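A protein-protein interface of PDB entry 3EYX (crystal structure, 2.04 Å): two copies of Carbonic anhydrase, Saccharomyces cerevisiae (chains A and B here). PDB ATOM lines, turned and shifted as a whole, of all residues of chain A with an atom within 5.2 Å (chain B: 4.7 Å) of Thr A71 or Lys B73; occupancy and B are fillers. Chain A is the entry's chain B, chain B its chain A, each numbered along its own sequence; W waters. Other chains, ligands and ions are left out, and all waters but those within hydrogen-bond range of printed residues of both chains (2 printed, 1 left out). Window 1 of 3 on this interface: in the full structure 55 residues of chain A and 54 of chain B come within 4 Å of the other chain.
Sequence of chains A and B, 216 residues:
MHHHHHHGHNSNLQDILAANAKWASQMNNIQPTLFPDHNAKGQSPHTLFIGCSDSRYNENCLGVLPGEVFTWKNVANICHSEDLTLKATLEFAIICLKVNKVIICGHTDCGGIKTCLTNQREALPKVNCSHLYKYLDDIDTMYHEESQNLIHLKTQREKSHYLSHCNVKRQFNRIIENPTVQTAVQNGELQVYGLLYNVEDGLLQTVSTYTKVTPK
The backbone carbonyl oxygen of Thr A71 sits at hydrogen-bond distance from the side-chain hydroxyl of Ser B53 (2.8 Å).
The side-chain amide nitrogen (ND2) of Asn B58 sits at hydrogen-bond distance from the side-chain carboxylate (OE2) of Glu A59, 2.7 Å away.
The backbone NH (N) of Lys B73 lies within hydrogen-bond range of the backbone carbonyl oxygen (O) of Lys A73, at 3.0 Å.
O of Trp B72 sits at hydrogen-bond distance from N of Gly B51 (3.0 Å).
The side-chain amino group (NZ) of Lys B73 sits at hydrogen-bond distance from the backbone carbonyl oxygen (O) of Ser B53 (3.2 Å).
The backbone carbonyl oxygen (O) of Asn B74 lies within hydrogen-bond range of the backbone NH (N) of Ser B53 (3.0 Å).
The backbone carbonyl oxygen (O) of Asp B54 sits at hydrogen-bond distance from the side-chain amino group (NZ) of Lys B73 (2.9 Å).
N of Trp A72 lies within hydrogen-bond range of O of Phe A49 (2.8 Å).
OE1 of Glu A59 sits close to OG1 of Thr A71.
Among the printed residues, merely in contact across the chains: Phe A70 with Ser B53 (3.3 Å), Phe A70 with Asp B54 (3.5 Å), Thr A71 with Lys B73 (3.6 Å), Trp A72 with Lys B73 (3.1 Å), Lys A73 with Thr B71 (3.6 Å) and Lys A73 with Trp B72 (3.2 Å).
Leu A48 touches none of the printed residues of chain B.
Of chain B, only Ser B53 and Lys B73 come within 4 Å of Thr A71.
Of the printed residues of chain B, Lys A73 touches Thr B71, Trp B72 and Lys B73.
Gly B51 touches none of the printed residues of chain A.
Printed residues of chain A within 4 Å of Thr B71: Lys A73 (3.6 Å).
Of the printed residues of chain A, Lys B73 touches Thr A71, Trp A72 and Lys A73.
The nearest printed residue of chain B that does not touch Phe A70 is Cys B52 (5.4 Å).
Of the 8 printed residues of chain A, 5 touch a printed residue of chain B.
Hydrophobic or aromatic side chains of chain A within 4 Å of the printed part of chain B: Phe A70 and Trp A72.
Hydrophobic or aromatic side chains of chain B within 4 Å of the printed part of chain A: Trp B72.
Among the printed residues, 9 pairs touch across the chains.
Thr A71 touches Lys B73, and with the chains exchanged Lys A73 touches Thr B71.
Trp A72 touches Lys B73, and with the chains exchanged Lys A73 touches Trp B72.
Lys A73 touches its own counterpart, Lys B73.
Of the 9 pairs that touch across the chains among the printed residues, 5 have their exchanged pair printed and touching as well.
Water W1 bridges NZ of Lys A73 and OG1 of Thr B71.
Water W2 bridges NE1 of Trp B72 and NE1 of Trp A72.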
ATOM      1  N   LEU A  48      17.152  25.902 -14.182  1.00  0.00           N
ATOM      2  CA  LEU A  48      18.175  26.927 -14.264  1.00  0.00           C
ATOM      3  C   LEU A  48      18.166  27.701 -12.943  1.00  0.00           C
ATOM      4  O   LEU A  48      17.155  28.290 -12.563  1.00  0.00           O
ATOM      5  CB  LEU A  48      17.940  27.899 -15.431  1.00  0.00           C
ATOM      6  CG  LEU A  48      18.818  29.175 -15.411  1.00  0.00           C
ATOM      7  CD1 LEU A  48      20.309  28.870 -15.617  1.00  0.00           C
ATOM      8  CD2 LEU A  48      18.326  30.208 -16.423  1.00  0.00           C
ATOM      9  N   PHE A  49      19.302  27.685 -12.263  1.00  0.00           N
ATOM     10  CA  PHE A  49      19.497  28.416 -11.017  1.00  0.00           C
ATOM     11  C   PHE A  49      20.416  29.599 -11.312  1.00  0.00           C
ATOM     12  O   PHE A  49      21.512  29.432 -11.880  1.00  0.00           O
ATOM     13  CB  PHE A  49      20.126  27.468  -9.992  1.00  0.00           C
ATOM     14  CG  PHE A  49      20.327  28.049  -8.601  1.00  0.00           C
ATOM     15  CD1 PHE A  49      19.347  27.905  -7.623  1.00  0.00           C
ATOM     16  CD2 PHE A  49      21.529  28.658  -8.256  1.00  0.00           C
ATOM     17  CE1 PHE A  49      19.568  28.386  -6.320  1.00  0.00           C
ATOM     18  CE2 PHE A  49      21.748  29.142  -6.972  1.00  0.00           C
ATOM     19  CZ  PHE A  49      20.781  29.012  -6.008  1.00  0.00           C
ATOM     20  N   GLU A  59      23.750  25.935  -6.082  1.00  0.00           N
ATOM     21  CA  GLU A  59      22.582  25.146  -6.467  1.00  0.00           C
ATOM     22  C   GLU A  59      22.272  23.991  -5.508  1.00  0.00           C
ATOM     23  O   GLU A  59      21.125  23.552  -5.415  1.00  0.00           O
ATOM     24  CB  GLU A  59      22.702  24.642  -7.919  1.00  0.00           C
ATOM     25  CG  GLU A  59      23.748  23.538  -8.158  1.00  0.00           C
ATOM     26  CD  GLU A  59      25.133  24.071  -8.471  1.00  0.00           C
ATOM     27  OE1 GLU A  59      25.444  25.228  -8.113  1.00  0.00           O
ATOM     28  OE2 GLU A  59      25.928  23.320  -9.077  1.00  0.00           O
ATOM     29  N   VAL A  69      20.563  20.645 -11.984  1.00  0.00           N
ATOM     30  CA  VAL A  69      20.495  22.112 -11.938  1.00  0.00           C
ATOM     31  C   VAL A  69      21.659  22.755 -12.696  1.00  0.00           C
ATOM     32  O   VAL A  69      22.831  22.611 -12.336  1.00  0.00           O
ATOM     33  CB  VAL A  69      20.428  22.669 -10.477  1.00  0.00           C
ATOM     34  CG1 VAL A  69      20.243  24.165 -10.500  1.00  0.00           C
ATOM     35  CG2 VAL A  69      19.290  22.025  -9.683  1.00  0.00           C
ATOM     36  N   PHE A  70      21.295  23.445 -13.770  1.00  0.00           N
ATOM     37  CA  PHE A  70      22.185  24.263 -14.583  1.00  0.00           C
ATOM     38  C   PHE A  70      22.268  25.660 -13.938  1.00  0.00           C
ATOM     39  O   PHE A  70      21.240  26.243 -13.601  1.00  0.00           O
ATOM     40  CB  PHE A  70      21.567  24.346 -15.978  1.00  0.00           C
ATOM     41  CG  PHE A  70      22.467  24.911 -17.028  1.00  0.00           C
ATOM     42  CD1 PHE A  70      23.482  24.137 -17.585  1.00  0.00           C
ATOM     43  CD2 PHE A  70      22.264  26.202 -17.509  1.00  0.00           C
ATOM     44  CE1 PHE A  70      24.294  24.648 -18.576  1.00  0.00           C
ATOM     45  CE2 PHE A  70      23.074  26.720 -18.504  1.00  0.00           C
ATOM     46  CZ  PHE A  70      24.097  25.940 -19.036  1.00  0.00           C
ATOM     47  N   THR A  71      23.476  26.197 -13.768  1.00  0.00           N
ATOM     48  CA  THR A  71      23.676  27.331 -12.847  1.00  0.00           C
ATOM     49  C   THR A  71      24.428  28.494 -13.458  1.00  0.00           C
ATOM     50  O   THR A  71      25.527  28.330 -13.994  1.00  0.00           O
ATOM     51  CB  THR A  71      24.411  26.881 -11.545  1.00  0.00           C
ATOM     52  OG1 THR A  71      23.626  25.906 -10.861  1.00  0.00           O
ATOM     53  CG2 THR A  71      24.694  28.065 -10.601  1.00  0.00           C
ATOM     54  N   TRP A  72      23.831  29.678 -13.361  1.00  0.00           N
ATOM     55  CA  TRP A  72      24.519  30.914 -13.688  1.00  0.00           C
ATOM     56  C   TRP A  72      24.793  31.633 -12.369  1.00  0.00           C
ATOM     57  O   TRP A  72      23.878  31.989 -11.647  1.00  0.00           O
ATOM     58  CB  TRP A  72      23.692  31.759 -14.676  1.00  0.00           C
ATOM     59  CG  TRP A  72      24.346  33.053 -15.105  1.00  0.00           C
ATOM     60  CD1 TRP A  72      25.682  33.310 -15.202  1.00  0.00           C
ATOM     61  CD2 TRP A  72      23.678  34.256 -15.516  1.00  0.00           C
ATOM     62  NE1 TRP A  72      25.892  34.602 -15.630  1.00  0.00           N
ATOM     63  CE2 TRP A  72      24.680  35.207 -15.823  1.00  0.00           C
ATOM     64  CE3 TRP A  72      22.329  34.629 -15.636  1.00  0.00           C
ATOM     65  CZ2 TRP A  72      24.380  36.513 -16.255  1.00  0.00           C
ATOM     66  CZ3 TRP A  72      22.031  35.941 -16.060  1.00  0.00           C
ATOM     67  CH2 TRP A  72      23.057  36.854 -16.370  1.00  0.00           C
ATOM     68  N   LYS A  73      26.066  31.792 -12.037  1.00  0.00           N
ATOM     69  CA  LYS A  73      26.446  32.353 -10.752  1.00  0.00           C
ATOM     70  C   LYS A  73      27.281  33.576 -11.066  1.00  0.00           C
ATOM     71  O   LYS A  73      28.328  33.445 -11.685  1.00  0.00           O
ATOM     72  CB  LYS A  73      27.285  31.334  -9.979  1.00  0.00           C
ATOM     73  CG  LYS A  73      26.843  31.044  -8.577  1.00  0.00           C
ATOM     74  CD  LYS A  73      27.902  30.148  -7.912  1.00  0.00           C
ATOM     75  CE  LYS A  73      27.506  29.721  -6.526  1.00  0.00           C
ATOM     76  NZ  LYS A  73      28.013  30.610  -5.475  1.00  0.00           N
ATOM     77  N   GLY B  51      33.893  28.383 -13.865  1.00  0.00           N
ATOM     78  CA  GLY B  51      33.527  27.132 -14.511  1.00  0.00           C
ATOM     79  C   GLY B  51      32.298  27.270 -15.373  1.00  0.00           C
ATOM     80  O   GLY B  51      31.645  28.316 -15.393  1.00  0.00           O
ATOM     81  N   CYS B  52      31.991  26.207 -16.103  1.00  0.00           N
ATOM     82  CA  CYS B  52      30.837  26.213 -16.975  1.00  0.00           C
ATOM     83  C   CYS B  52      29.568  26.058 -16.146  1.00  0.00           C
ATOM     84  O   CYS B  52      29.597  25.437 -15.085  1.00  0.00           O
ATOM     85  CB  CYS B  52      30.935  25.076 -17.981  1.00  0.00           C
ATOM     86  SG  CYS B  52      29.626  25.135 -19.179  1.00  0.00           S
ATOM     87  N   SER B  53      28.465  26.612 -16.648  1.00  0.00           N
ATOM     88  CA  SER B  53      27.145  26.464 -16.028  1.00  0.00           C
ATOM     89  C   SER B  53      26.660  25.015 -15.993  1.00  0.00           C
ATOM     90  O   SER B  53      25.738  24.683 -15.243  1.00  0.00           O
ATOM     91  CB  SER B  53      26.115  27.334 -16.751  1.00  0.00           C
ATOM     92  OG  SER B  53      26.438  28.712 -16.649  1.00  0.00           O
ATOM     93  N   ASP B  54      27.277  24.163 -16.810  1.00  0.00           N
ATOM     94  CA  ASP B  54      26.983  22.723 -16.832  1.00  0.00           C
ATOM     95  C   ASP B  54      26.594  22.147 -15.465  1.00  0.00           C
ATOM     96  O   ASP B  54      27.305  22.334 -14.475  1.00  0.00           O
ATOM     97  CB  ASP B  54      28.170  21.947 -17.416  1.00  0.00           C
ATOM     98  CG  ASP B  54      27.789  20.535 -17.853  1.00  0.00           C
ATOM     99  OD1 ASP B  54      27.532  19.676 -16.986  1.00  0.00           O
ATOM    100  OD2 ASP B  54      27.760  20.285 -19.064  1.00  0.00           O
ATOM    101  N   TYR B  57      28.914  19.572 -12.752  1.00  0.00           N
ATOM    102  CA  TYR B  57      29.958  19.944 -11.813  1.00  0.00           C
ATOM    103  C   TYR B  57      29.844  21.393 -11.345  1.00  0.00           C
ATOM    104  O   TYR B  57      29.115  22.195 -11.922  1.00  0.00           O
ATOM    105  CB  TYR B  57      31.358  19.666 -12.402  1.00  0.00           C
ATOM    106  CG  TYR B  57      31.896  20.712 -13.365  1.00  0.00           C
ATOM    107  CD1 TYR B  57      33.141  21.305 -13.144  1.00  0.00           C
ATOM    108  CD2 TYR B  57      31.167  21.110 -14.500  1.00  0.00           C
ATOM    109  CE1 TYR B  57      33.651  22.255 -14.021  1.00  0.00           C
ATOM    110  CE2 TYR B  57      31.666  22.073 -15.378  1.00  0.00           C
ATOM    111  CZ  TYR B  57      32.911  22.636 -15.132  1.00  0.00           C
ATOM    112  OH  TYR B  57      33.431  23.577 -15.990  1.00  0.00           O
ATOM    113  N   ASN B  58      30.578  21.688 -10.279  1.00  0.00           N
ATOM    114  CA  ASN B  58      30.731  23.036  -9.742  1.00  0.00           C
ATOM    115  C   ASN B  58      32.007  23.079  -8.914  1.00  0.00           C
ATOM    116  O   ASN B  58      32.872  22.203  -9.055  1.00  0.00           O
ATOM    117  CB  ASN B  58      29.490  23.464  -8.933  1.00  0.00           C
ATOM    118  CG  ASN B  58      29.134  22.486  -7.808  1.00  0.00           C
ATOM    119  OD1 ASN B  58      29.989  21.756  -7.303  1.00  0.00           O
ATOM    120  ND2 ASN B  58      27.860  22.487  -7.405  1.00  0.00           N
ATOM    121  N   THR B  71      32.506  31.648  -6.649  1.00  0.00           N
ATOM    122  CA  THR B  71      32.325  31.053  -7.991  1.00  0.00           C
ATOM    123  C   THR B  71      31.637  31.905  -9.065  1.00  0.00           C
ATOM    124  O   THR B  71      30.533  32.405  -8.876  1.00  0.00           O
ATOM    125  CB  THR B  71      31.595  29.682  -7.885  1.00  0.00           C
ATOM    126  OG1 THR B  71      32.398  28.799  -7.105  1.00  0.00           O
ATOM    127  CG2 THR B  71      31.335  29.047  -9.267  1.00  0.00           C
ATOM    128  N   TRP B  72      32.305  32.040 -10.205  1.00  0.00           N
ATOM    129  CA  TRP B  72      31.683  32.574 -11.409  1.00  0.00           C
ATOM    130  C   TRP B  72      31.395  31.414 -12.361  1.00  0.00           C
ATOM    131  O   TRP B  72      32.308  30.771 -12.870  1.00  0.00           O
ATOM    132  CB  TRP B  72      32.608  33.591 -12.061  1.00  0.00           C
ATOM    133  CG  TRP B  72      32.037  34.304 -13.261  1.00  0.00           C
ATOM    134  CD1 TRP B  72      30.718  34.526 -13.545  1.00  0.00           C
ATOM    135  CD2 TRP B  72      32.783  34.916 -14.319  1.00  0.00           C
ATOM    136  NE1 TRP B  72      30.598  35.226 -14.721  1.00  0.00           N
ATOM    137  CE2 TRP B  72      31.848  35.483 -15.215  1.00  0.00           C
ATOM    138  CE3 TRP B  72      34.152  35.039 -14.597  1.00  0.00           C
ATOM    139  CZ2 TRP B  72      32.237  36.160 -16.373  1.00  0.00           C
ATOM    140  CZ3 TRP B  72      34.536  35.705 -15.744  1.00  0.00           C
ATOM    141  CH2 TRP B  72      33.581  36.267 -16.618  1.00  0.00           C
ATOM    142  N   LYS B  73      30.118  31.163 -12.606  1.00  0.00           N
ATOM    143  CA  LYS B  73      29.691  30.015 -13.406  1.00  0.00           C
ATOM    144  C   LYS B  73      28.915  30.548 -14.597  1.00  0.00           C
ATOM    145  O   LYS B  73      27.909  31.233 -14.413  1.00  0.00           O
ATOM    146  CB  LYS B  73      28.796  29.123 -12.556  1.00  0.00           C
ATOM    147  CG  LYS B  73      29.109  27.645 -12.584  1.00  0.00           C
ATOM    148  CD  LYS B  73      27.994  26.909 -11.859  1.00  0.00           C
ATOM    149  CE  LYS B  73      28.279  25.433 -11.699  1.00  0.00           C
ATOM    150  NZ  LYS B  73      27.927  24.653 -12.913  1.00  0.00           N
ATOM    151  N   ASN B  74      29.397  30.273 -15.815  1.00  0.00           N
ATOM    152  CA  ASN B  74      28.730  30.763 -17.027  1.00  0.00           C
ATOM    153  C   ASN B  74      28.830  29.788 -18.197  1.00  0.00           C
ATOM    154  O   ASN B  74      29.701  28.909 -18.206  1.00  0.00           O
ATOM    155  CB  ASN B  74      29.211  32.176 -17.421  1.00  0.00           C
ATOM    156  CG  ASN B  74      30.614  32.194 -18.040  1.00  0.00           C
ATOM    157  OD1 ASN B  74      30.866  31.565 -19.063  1.00  0.00           O
ATOM    158  ND2 ASN B  74      31.518  32.965 -17.434  1.00  0.00           N
HETATM  159  O   HOH W   1      30.420  29.460  -4.738  1.00  0.00           O
HETATM  160  O   HOH W   2      28.367  36.261 -16.277  1.00  0.00           O
